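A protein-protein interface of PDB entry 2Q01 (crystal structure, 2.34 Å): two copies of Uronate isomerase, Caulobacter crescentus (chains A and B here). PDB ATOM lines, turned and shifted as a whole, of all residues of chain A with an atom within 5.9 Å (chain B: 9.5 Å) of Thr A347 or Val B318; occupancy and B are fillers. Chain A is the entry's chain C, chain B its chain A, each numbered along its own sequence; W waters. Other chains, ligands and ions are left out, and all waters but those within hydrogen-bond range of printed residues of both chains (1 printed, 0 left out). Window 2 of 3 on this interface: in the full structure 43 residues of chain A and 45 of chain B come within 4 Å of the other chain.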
ATOM      1  N   LEU A 342     -12.180 -34.092 -25.935  1.00  0.00           N
ATOM      2  CA  LEU A 342     -13.016 -33.054 -26.537  1.00  0.00           C
ATOM      3  C   LEU A 342     -12.244 -31.858 -27.062  1.00  0.00           C
ATOM      4  O   LEU A 342     -12.820 -31.012 -27.759  1.00  0.00           O
ATOM      5  CB  LEU A 342     -14.058 -32.562 -25.530  1.00  0.00           C
ATOM      6  CG  LEU A 342     -15.189 -33.521 -25.176  1.00  0.00           C
ATOM      7  CD1 LEU A 342     -15.991 -32.941 -24.029  1.00  0.00           C
ATOM      8  CD2 LEU A 342     -16.076 -33.779 -26.381  1.00  0.00           C
ATOM      9  N   LYS A 343     -10.953 -31.788 -26.738  1.00  0.00           N
ATOM     10  CA  LYS A 343     -10.127 -30.631 -27.093  1.00  0.00           C
ATOM     11  C   LYS A 343     -10.062 -30.232 -28.588  1.00  0.00           C
ATOM     12  O   LYS A 343     -10.189 -29.039 -28.877  1.00  0.00           O
ATOM     13  CB  LYS A 343      -8.734 -30.697 -26.452  1.00  0.00           C
ATOM     14  CG  LYS A 343      -8.052 -29.345 -26.421  1.00  0.00           C
ATOM     15  CD  LYS A 343      -6.660 -29.388 -25.857  1.00  0.00           C
ATOM     16  CE  LYS A 343      -6.042 -28.003 -25.938  1.00  0.00           C
ATOM     17  NZ  LYS A 343      -4.702 -27.939 -25.294  1.00  0.00           N
ATOM     18  N   PRO A 344      -9.859 -31.198 -29.529  1.00  0.00           N
ATOM     19  CA  PRO A 344      -9.921 -30.836 -30.961  1.00  0.00           C
ATOM     20  C   PRO A 344     -11.197 -30.118 -31.426  1.00  0.00           C
ATOM     21  O   PRO A 344     -11.105 -29.101 -32.114  1.00  0.00           O
ATOM     22  CB  PRO A 344      -9.789 -32.190 -31.670  1.00  0.00           C
ATOM     23  CG  PRO A 344      -8.996 -32.996 -30.739  1.00  0.00           C
ATOM     24  CD  PRO A 344      -9.505 -32.624 -29.375  1.00  0.00           C
ATOM     25  N   LEU A 345     -12.363 -30.641 -31.050  1.00  0.00           N
ATOM     26  CA  LEU A 345     -13.649 -30.013 -31.373  1.00  0.00           C
ATOM     27  C   LEU A 345     -13.823 -28.657 -30.691  1.00  0.00           C
ATOM     28  O   LEU A 345     -14.337 -27.719 -31.296  1.00  0.00           O
ATOM     29  CB  LEU A 345     -14.808 -30.941 -30.998  1.00  0.00           C
ATOM     30  CG  LEU A 345     -16.259 -30.490 -31.205  1.00  0.00           C
ATOM     31  CD1 LEU A 345     -16.524 -30.057 -32.633  1.00  0.00           C
ATOM     32  CD2 LEU A 345     -17.202 -31.597 -30.815  1.00  0.00           C
ATOM     33  N   LEU A 346     -13.384 -28.562 -29.438  1.00  0.00           N
ATOM     34  CA  LEU A 346     -13.492 -27.322 -28.671  1.00  0.00           C
ATOM     35  C   LEU A 346     -12.505 -26.243 -29.121  1.00  0.00           C
ATOM     36  O   LEU A 346     -12.717 -25.061 -28.855  1.00  0.00           O
ATOM     37  CB  LEU A 346     -13.355 -27.593 -27.166  1.00  0.00           C
ATOM     38  CG  LEU A 346     -14.500 -28.343 -26.468  1.00  0.00           C
ATOM     39  CD1 LEU A 346     -14.111 -28.700 -25.040  1.00  0.00           C
ATOM     40  CD2 LEU A 346     -15.810 -27.557 -26.493  1.00  0.00           C
ATOM     41  N   THR A 347     -11.436 -26.649 -29.805  1.00  0.00           N
ATOM     42  CA  THR A 347     -10.474 -25.705 -30.380  1.00  0.00           C
ATOM     43  C   THR A 347     -11.106 -25.022 -31.591  1.00  0.00           C
ATOM     44  O   THR A 347     -10.965 -23.810 -31.783  1.00  0.00           O
ATOM     45  CB  THR A 347      -9.139 -26.412 -30.752  1.00  0.00           C
ATOM     46  OG1 THR A 347      -8.536 -26.945 -29.564  1.00  0.00           O
ATOM     47  CG2 THR A 347      -8.154 -25.458 -31.424  1.00  0.00           C
ATOM     48  N   ARG A 348     -11.836 -25.806 -32.380  1.00  0.00           N
ATOM     49  CA  ARG A 348     -12.457 -25.320 -33.604  1.00  0.00           C
ATOM     50  C   ARG A 348     -13.746 -24.540 -33.345  1.00  0.00           C
ATOM     51  O   ARG A 348     -13.928 -23.441 -33.868  1.00  0.00           O
ATOM     52  CB  ARG A 348     -12.735 -26.494 -34.546  1.00  0.00           C
ATOM     53  CG  ARG A 348     -13.210 -26.087 -35.929  1.00  0.00           C
ATOM     54  CD  ARG A 348     -13.697 -27.302 -36.702  1.00  0.00           C
ATOM     55  NE  ARG A 348     -14.291 -26.925 -37.982  1.00  0.00           N
ATOM     56  CZ  ARG A 348     -13.630 -26.878 -39.135  1.00  0.00           C
ATOM     57  NH1 ARG A 348     -12.342 -27.192 -39.186  1.00  0.00           N
ATOM     58  NH2 ARG A 348     -14.263 -26.520 -40.244  1.00  0.00           N
ATOM     59  N   LEU A 349     -14.633 -25.117 -32.535  1.00  0.00           N
ATOM     60  CA  LEU A 349     -16.007 -24.629 -32.408  1.00  0.00           C
ATOM     61  C   LEU A 349     -16.468 -24.361 -30.976  1.00  0.00           C
ATOM     62  O   LEU A 349     -17.662 -24.209 -30.739  1.00  0.00           O
ATOM     63  CB  LEU A 349     -16.973 -25.631 -33.051  1.00  0.00           C
ATOM     64  CG  LEU A 349     -16.786 -26.050 -34.506  1.00  0.00           C
ATOM     65  CD1 LEU A 349     -17.715 -27.201 -34.846  1.00  0.00           C
ATOM     66  CD2 LEU A 349     -17.012 -24.867 -35.431  1.00  0.00           C
ATOM     67  N   GLY A 350     -15.535 -24.284 -30.032  1.00  0.00           N
ATOM     68  CA  GLY A 350     -15.882 -24.218 -28.609  1.00  0.00           C
ATOM     69  C   GLY A 350     -16.426 -22.906 -28.076  1.00  0.00           C
ATOM     70  O   GLY A 350     -16.890 -22.843 -26.936  1.00  0.00           O
ATOM     71  N   ASN A 351     -16.360 -21.855 -28.889  1.00  0.00           N
ATOM     72  CA  ASN A 351     -16.862 -20.540 -28.493  1.00  0.00           C
ATOM     73  C   ASN A 351     -17.953 -20.053 -29.450  1.00  0.00           C
ATOM     74  O   ASN A 351     -18.417 -18.915 -29.352  1.00  0.00           O
ATOM     75  CB  ASN A 351     -15.717 -19.522 -28.398  1.00  0.00           C
ATOM     76  CG  ASN A 351     -14.419 -20.137 -27.885  1.00  0.00           C
ATOM     77  OD1 ASN A 351     -13.674 -20.770 -28.640  1.00  0.00           O
ATOM     78  ND2 ASN A 351     -14.141 -19.951 -26.599  1.00  0.00           N
ATOM     79  N   TYR A 378     -17.001 -23.401 -21.268  1.00  0.00           N
ATOM     80  CA  TYR A 378     -17.281 -23.327 -22.704  1.00  0.00           C
ATOM     81  C   TYR A 378     -18.722 -22.968 -22.967  1.00  0.00           C
ATOM     82  O   TYR A 378     -19.615 -23.656 -22.470  1.00  0.00           O
ATOM     83  CB  TYR A 378     -16.920 -24.635 -23.422  1.00  0.00           C
ATOM     84  CG  TYR A 378     -15.434 -24.809 -23.593  1.00  0.00           C
ATOM     85  CD1 TYR A 378     -14.685 -25.502 -22.646  1.00  0.00           C
ATOM     86  CD2 TYR A 378     -14.769 -24.251 -24.683  1.00  0.00           C
ATOM     87  CE1 TYR A 378     -13.316 -25.647 -22.786  1.00  0.00           C
ATOM     88  CE2 TYR A 378     -13.397 -24.395 -24.837  1.00  0.00           C
ATOM     89  CZ  TYR A 378     -12.680 -25.092 -23.882  1.00  0.00           C
ATOM     90  OH  TYR A 378     -11.327 -25.245 -24.025  1.00  0.00           O
ATOM     91  N   TYR B  74     -18.735 -16.093 -19.110  1.00  0.00           N
ATOM     92  CA  TYR B  74     -18.234 -16.492 -20.431  1.00  0.00           C
ATOM     93  C   TYR B  74     -18.892 -17.787 -20.867  1.00  0.00           C
ATOM     94  O   TYR B  74     -19.242 -17.962 -22.033  1.00  0.00           O
ATOM     95  CB  TYR B  74     -16.717 -16.684 -20.407  1.00  0.00           C
ATOM     96  CG  TYR B  74     -16.099 -16.924 -21.770  1.00  0.00           C
ATOM     97  CD1 TYR B  74     -15.905 -15.871 -22.659  1.00  0.00           C
ATOM     98  CD2 TYR B  74     -15.703 -18.203 -22.168  1.00  0.00           C
ATOM     99  CE1 TYR B  74     -15.340 -16.080 -23.909  1.00  0.00           C
ATOM    100  CE2 TYR B  74     -15.135 -18.421 -23.419  1.00  0.00           C
ATOM    101  CZ  TYR B  74     -14.954 -17.350 -24.281  1.00  0.00           C
ATOM    102  OH  TYR B  74     -14.398 -17.536 -25.524  1.00  0.00           O
ATOM    103  N   LYS B  88      -4.711  -9.422 -24.052  1.00  0.00           N
ATOM    104  CA  LYS B  88      -3.299  -9.307 -24.423  1.00  0.00           C
ATOM    105  C   LYS B  88      -3.051  -7.932 -25.041  1.00  0.00           C
ATOM    106  O   LYS B  88      -1.911  -7.466 -25.113  1.00  0.00           O
ATOM    107  CB  LYS B  88      -2.891 -10.425 -25.386  1.00  0.00           C
ATOM    108  CG  LYS B  88      -1.492 -10.965 -25.155  1.00  0.00           C
ATOM    109  CD  LYS B  88      -1.387 -12.419 -25.588  1.00  0.00           C
ATOM    110  CE  LYS B  88      -0.079 -13.033 -25.113  1.00  0.00           C
ATOM    111  NZ  LYS B  88      -0.032 -14.502 -25.347  1.00  0.00           N
ATOM    112  N   GLU B 208       5.836 -21.303 -22.788  1.00  0.00           N
ATOM    113  CA  GLU B 208       6.140 -20.335 -23.848  1.00  0.00           C
ATOM    114  C   GLU B 208       6.954 -19.141 -23.346  1.00  0.00           C
ATOM    115  O   GLU B 208       7.697 -18.519 -24.111  1.00  0.00           O
ATOM    116  CB  GLU B 208       4.858 -19.846 -24.537  1.00  0.00           C
ATOM    117  CG  GLU B 208       3.728 -19.446 -23.594  1.00  0.00           C
ATOM    118  CD  GLU B 208       2.744 -20.574 -23.369  1.00  0.00           C
ATOM    119  OE1 GLU B 208       1.858 -20.768 -24.225  1.00  0.00           O
ATOM    120  OE2 GLU B 208       2.857 -21.270 -22.339  1.00  0.00           O
ATOM    121  N   HIS B 313      -4.463 -29.058 -16.523  1.00  0.00           N
ATOM    122  CA  HIS B 313      -4.312 -28.871 -17.966  1.00  0.00           C
ATOM    123  C   HIS B 313      -4.525 -27.402 -18.252  1.00  0.00           C
ATOM    124  O   HIS B 313      -5.645 -26.973 -18.552  1.00  0.00           O
ATOM    125  CB  HIS B 313      -5.368 -29.686 -18.721  1.00  0.00           C
ATOM    126  CG  HIS B 313      -5.118 -29.814 -20.196  1.00  0.00           C
ATOM    127  ND1 HIS B 313      -5.001 -28.727 -21.036  1.00  0.00           N
ATOM    128  CD2 HIS B 313      -5.002 -30.909 -20.985  1.00  0.00           C
ATOM    129  CE1 HIS B 313      -4.809 -29.146 -22.273  1.00  0.00           C
ATOM    130  NE2 HIS B 313      -4.806 -30.466 -22.270  1.00  0.00           N
ATOM    131  N   ARG B 314      -3.443 -26.632 -18.173  1.00  0.00           N
ATOM    132  CA  ARG B 314      -3.518 -25.182 -18.338  1.00  0.00           C
ATOM    133  C   ARG B 314      -3.763 -24.795 -19.788  1.00  0.00           C
ATOM    134  O   ARG B 314      -3.325 -25.496 -20.704  1.00  0.00           O
ATOM    135  CB  ARG B 314      -2.257 -24.499 -17.789  1.00  0.00           C
ATOM    136  CG  ARG B 314      -1.926 -24.917 -16.361  1.00  0.00           C
ATOM    137  CD  ARG B 314      -1.162 -23.857 -15.584  1.00  0.00           C
ATOM    138  NE  ARG B 314      -0.864 -24.326 -14.229  1.00  0.00           N
ATOM    139  CZ  ARG B 314      -1.655 -24.145 -13.172  1.00  0.00           C
ATOM    140  NH1 ARG B 314      -2.800 -23.488 -13.297  1.00  0.00           N
ATOM    141  NH2 ARG B 314      -1.296 -24.619 -11.984  1.00  0.00           N
ATOM    142  N   ASN B 315      -4.490 -23.692 -19.965  1.00  0.00           N
ATOM    143  CA  ASN B 315      -4.760 -23.080 -21.269  1.00  0.00           C
ATOM    144  C   ASN B 315      -5.430 -24.038 -22.251  1.00  0.00           C
ATOM    145  O   ASN B 315      -4.965 -24.221 -23.376  1.00  0.00           O
ATOM    146  CB  ASN B 315      -3.484 -22.456 -21.865  1.00  0.00           C
ATOM    147  CG  ASN B 315      -2.676 -21.673 -20.837  1.00  0.00           C
ATOM    148  OD1 ASN B 315      -3.204 -20.805 -20.134  1.00  0.00           O
ATOM    149  ND2 ASN B 315      -1.388 -21.982 -20.744  1.00  0.00           N
ATOM    150  N   HIS B 316      -6.521 -24.647 -21.794  1.00  0.00           N
ATOM    151  CA  HIS B 316      -7.290 -25.624 -22.565  1.00  0.00           C
ATOM    152  C   HIS B 316      -8.017 -24.958 -23.737  1.00  0.00           C
ATOM    153  O   HIS B 316      -8.183 -25.571 -24.795  1.00  0.00           O
ATOM    154  CB  HIS B 316      -8.278 -26.326 -21.631  1.00  0.00           C
ATOM    155  CG  HIS B 316      -8.956 -27.519 -22.228  1.00  0.00           C
ATOM    156  ND1 HIS B 316     -10.169 -27.439 -22.879  1.00  0.00           N
ATOM    157  CD2 HIS B 316      -8.606 -28.825 -22.246  1.00  0.00           C
ATOM    158  CE1 HIS B 316     -10.529 -28.643 -23.286  1.00  0.00           C
ATOM    159  NE2 HIS B 316      -9.599 -29.503 -22.911  1.00  0.00           N
ATOM    160  N   ASN B 317      -8.439 -23.706 -23.538  1.00  0.00           N
ATOM    161  CA  ASN B 317      -9.022 -22.886 -24.602  1.00  0.00           C
ATOM    162  C   ASN B 317      -7.898 -22.224 -25.392  1.00  0.00           C
ATOM    163  O   ASN B 317      -7.320 -21.227 -24.945  1.00  0.00           O
ATOM    164  CB  ASN B 317      -9.964 -21.830 -24.008  1.00  0.00           C
ATOM    165  CG  ASN B 317     -11.042 -21.358 -24.990  1.00  0.00           C
ATOM    166  OD1 ASN B 317     -12.220 -21.332 -24.647  1.00  0.00           O
ATOM    167  ND2 ASN B 317     -10.642 -20.957 -26.195  1.00  0.00           N
ATOM    168  N   VAL B 318      -7.607 -22.789 -26.563  1.00  0.00           N
ATOM    169  CA  VAL B 318      -6.477 -22.372 -27.397  1.00  0.00           C
ATOM    170  C   VAL B 318      -6.659 -20.943 -27.920  1.00  0.00           C
ATOM    171  O   VAL B 318      -5.763 -20.109 -27.769  1.00  0.00           O
ATOM    172  CB  VAL B 318      -6.228 -23.372 -28.562  1.00  0.00           C
ATOM    173  CG1 VAL B 318      -5.001 -22.978 -29.377  1.00  0.00           C
ATOM    174  CG2 VAL B 318      -6.059 -24.781 -28.022  1.00  0.00           C
ATOM    175  N   GLY B 319      -7.829 -20.667 -28.501  1.00  0.00           N
ATOM    176  CA  GLY B 319      -8.170 -19.332 -29.002  1.00  0.00           C
ATOM    177  C   GLY B 319      -8.131 -18.224 -27.957  1.00  0.00           C
ATOM    178  O   GLY B 319      -7.775 -17.083 -28.266  1.00  0.00           O
ATOM    179  N   LEU B 320      -8.493 -18.569 -26.723  1.00  0.00           N
ATOM    180  CA  LEU B 320      -8.483 -17.637 -25.599  1.00  0.00           C
ATOM    181  C   LEU B 320      -7.067 -17.344 -25.110  1.00  0.00           C
ATOM    182  O   LEU B 320      -6.779 -16.239 -24.643  1.00  0.00           O
ATOM    183  CB  LEU B 320      -9.327 -18.198 -24.454  1.00  0.00           C
ATOM    184  CG  LEU B 320      -9.603 -17.338 -23.220  1.00  0.00           C
ATOM    185  CD1 LEU B 320     -10.544 -16.200 -23.571  1.00  0.00           C
ATOM    186  CD2 LEU B 320     -10.179 -18.196 -22.117  1.00  0.00           C
ATOM    187  N   LEU B 321      -6.195 -18.344 -25.212  1.00  0.00           N
ATOM    188  CA  LEU B 321      -4.783 -18.202 -24.855  1.00  0.00           C
ATOM    189  C   LEU B 321      -4.081 -17.218 -25.796  1.00  0.00           C
ATOM    190  O   LEU B 321      -3.261 -16.408 -25.359  1.00  0.00           O
ATOM    191  CB  LEU B 321      -4.092 -19.577 -24.871  1.00  0.00           C
ATOM    192  CG  LEU B 321      -2.563 -19.688 -24.830  1.00  0.00           C
ATOM    193  CD1 LEU B 321      -1.994 -19.254 -23.482  1.00  0.00           C
ATOM    194  CD2 LEU B 321      -2.127 -21.106 -25.171  1.00  0.00           C
ATOM    195  N   ASN B 322      -4.427 -17.290 -27.080  1.00  0.00           N
ATOM    196  CA  ASN B 322      -3.885 -16.389 -28.095  1.00  0.00           C
ATOM    197  C   ASN B 322      -4.387 -14.957 -27.927  1.00  0.00           C
ATOM    198  O   ASN B 322      -3.624 -14.004 -28.105  1.00  0.00           O
ATOM    199  CB  ASN B 322      -4.207 -16.904 -29.503  1.00  0.00           C
ATOM    200  CG  ASN B 322      -3.634 -18.293 -29.768  1.00  0.00           C
ATOM    201  OD1 ASN B 322      -2.485 -18.588 -29.418  1.00  0.00           O
ATOM    202  ND2 ASN B 322      -4.435 -19.152 -30.394  1.00  0.00           N
ATOM    203  N   SER B 323      -5.663 -14.821 -27.566  1.00  0.00           N
ATOM    204  CA  SER B 323      -6.302 -13.513 -27.420  1.00  0.00           C
ATOM    205  C   SER B 323      -6.055 -12.838 -26.066  1.00  0.00           C
ATOM    206  O   SER B 323      -5.781 -11.641 -26.024  1.00  0.00           O
ATOM    207  CB  SER B 323      -7.805 -13.595 -27.723  1.00  0.00           C
ATOM    208  OG  SER B 323      -8.482 -14.416 -26.787  1.00  0.00           O
ATOM    209  N   HIS B 324      -6.145 -13.598 -24.974  1.00  0.00           N
ATOM    210  CA  HIS B 324      -6.079 -13.026 -23.619  1.00  0.00           C
ATOM    211  C   HIS B 324      -4.893 -13.495 -22.774  1.00  0.00           C
ATOM    212  O   HIS B 324      -4.422 -12.752 -21.910  1.00  0.00           O
ATOM    213  CB  HIS B 324      -7.377 -13.296 -22.852  1.00  0.00           C
ATOM    214  CG  HIS B 324      -8.566 -12.548 -23.374  1.00  0.00           C
ATOM    215  ND1 HIS B 324      -9.189 -12.872 -24.561  1.00  0.00           N
ATOM    216  CD2 HIS B 324      -9.261 -11.508 -22.857  1.00  0.00           C
ATOM    217  CE1 HIS B 324     -10.206 -12.053 -24.761  1.00  0.00           C
ATOM    218  NE2 HIS B 324     -10.270 -11.215 -23.743  1.00  0.00           N
ATOM    219  N   GLY B 325      -4.434 -14.727 -22.994  1.00  0.00           N
ATOM    220  CA  GLY B 325      -3.266 -15.253 -22.272  1.00  0.00           C
ATOM    221  C   GLY B 325      -3.557 -16.229 -21.145  1.00  0.00           C
ATOM    222  O   GLY B 325      -4.555 -16.945 -21.170  1.00  0.00           O
ATOM    223  N   ARG B 326      -2.668 -16.249 -20.156  1.00  0.00           N
ATOM    224  CA  ARG B 326      -2.734 -17.189 -19.036  1.00  0.00           C
ATOM    225  C   ARG B 326      -3.668 -16.745 -17.908  1.00  0.00           C
ATOM    226  O   ARG B 326      -3.995 -15.559 -17.798  1.00  0.00           O
ATOM    227  CB  ARG B 326      -1.334 -17.416 -18.465  1.00  0.00           C
ATOM    228  CG  ARG B 326      -0.611 -18.598 -19.052  1.00  0.00           C
ATOM    229  CD  ARG B 326       0.554 -18.994 -18.163  1.00  0.00           C
ATOM    230  NE  ARG B 326       0.891 -20.414 -18.280  1.00  0.00           N
ATOM    231  CZ  ARG B 326       1.710 -20.925 -19.199  1.00  0.00           C
ATOM    232  NH1 ARG B 326       1.954 -22.231 -19.215  1.00  0.00           N
ATOM    233  NH2 ARG B 326       2.284 -20.135 -20.100  1.00  0.00           N
ATOM    234  N   ALA B 330      -9.467 -21.157 -18.004  1.00  0.00           N
ATOM    235  CA  ALA B 330      -9.549 -22.321 -18.879  1.00  0.00           C
ATOM    236  C   ALA B 330      -8.548 -23.404 -18.484  1.00  0.00           C
ATOM    237  O   ALA B 330      -8.065 -24.147 -19.336  1.00  0.00           O
ATOM    238  CB  ALA B 330      -9.338 -21.905 -20.317  1.00  0.00           C
ATOM    239  N   ASP B 331      -8.231 -23.484 -17.192  1.00  0.00           N
ATOM    240  CA  ASP B 331      -7.311 -24.498 -16.678  1.00  0.00           C
ATOM    241  C   ASP B 331      -8.108 -25.650 -16.051  1.00  0.00           C
ATOM    242  O   ASP B 331      -8.616 -25.537 -14.932  1.00  0.00           O
ATOM    243  CB  ASP B 331      -6.339 -23.888 -15.661  1.00  0.00           C
ATOM    244  CG  ASP B 331      -5.502 -22.736 -16.233  1.00  0.00           C
ATOM    245  OD1 ASP B 331      -5.747 -22.279 -17.369  1.00  0.00           O
ATOM    246  OD2 ASP B 331      -4.584 -22.281 -15.522  1.00  0.00           O
ATOM    247  N   ILE B 332      -8.199 -26.754 -16.788  1.00  0.00           N
ATOM    248  CA  ILE B 332      -9.073 -27.883 -16.457  1.00  0.00           C
ATOM    249  C   ILE B 332      -8.275 -28.989 -15.765  1.00  0.00           C
ATOM    250  O   ILE B 332      -7.165 -29.281 -16.173  1.00  0.00           O
ATOM    251  CB  ILE B 332      -9.746 -28.450 -17.751  1.00  0.00           C
ATOM    252  CG1 ILE B 332     -10.248 -27.321 -18.669  1.00  0.00           C
ATOM    253  CG2 ILE B 332     -10.871 -29.439 -17.438  1.00  0.00           C
ATOM    254  CD1 ILE B 332     -11.326 -26.406 -18.096  1.00  0.00           C
HETATM  255  O   HOH W   1      -9.337 -25.451 -27.211  1.00  0.00           O
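ND1 of His B316 is in hydrogen-bond range of OH of Tyr A378, at 2.7 Å. ND2 of Asn A351 sits at hydrogen-bond distance from OD1 of Asn B317 (3.1 Å). OH of Tyr B74 lies within hydrogen-bond range of ND2 of Asn A351 (2.7 Å). N of Asn B317 lies within hydrogen-bond range of OH of Tyr A378, 3.3 Å away.
No position is printed for both chains.
Among the printed residues, merely in contact across the chains: Lys A343 with His B313 (3.3 Å), Lys A343 with His B316 (3.4 Å), Lys A343 with Val B318 (3.8 Å), Leu A346 with His B316 (3.99 Å) and Thr A347 with Val B318 (3.6 Å).
Water W1 lies within hydrogen-bond range of the backbone carbonyl oxygen of His B316 (2.7 Å), the side-chain hydroxyl of Thr A347 (2.9 Å) and the backbone NH of Val B318 (3.2 Å).
Printed residues of chain B that touch a printed residue of chain A: Tyr B74, His B313, His B316, Asn B317 and Val B318. Among the printed residues, no Asp or Glu carboxylate lies within 4 Å of a Lys or Arg side-chain nitrogen of the other chain.
O of Lys A343 lies within hydrogen-bond range of OG1 of Thr A347, 2.8 Å away. N of His B313 lies within hydrogen-bond range of O of Ile B332 (2.7 Å). N of His B316 lies within hydrogen-bond range of O of Ala B330. O of Val B318 sits at hydrogen-bond distance from ND2 of Asn B322, at 3.1 Å. The side-chain amide nitrogen of Asn B317 sits close to the backbone NH of Leu B320 (3.3 Å).
Of the printed residues of chain B, Lys A343 touches His B313, His B316 and Val B318. Of the printed residues of chain B, Asn A351 touches Tyr B74 (2.7 Å) and Asn B317 (3.1 Å). Printed residues of chain B within 4 Å of Tyr A378: His B316 (2.7 Å) and Asn B317 (3.3 Å). Of the printed residues of chain A, His B313 touches Lys A343 (3.3 Å). Of the printed residues of chain A, Asn B317 touches Asn A351 and Tyr A378. Of chain A, only Lys A343 (3.8 Å) and Thr A347 (3.6 Å) come within 4 Å of Val B318. The nearest residue of chain A that does not touch Val B318 is Tyr A378 (5.1 Å).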
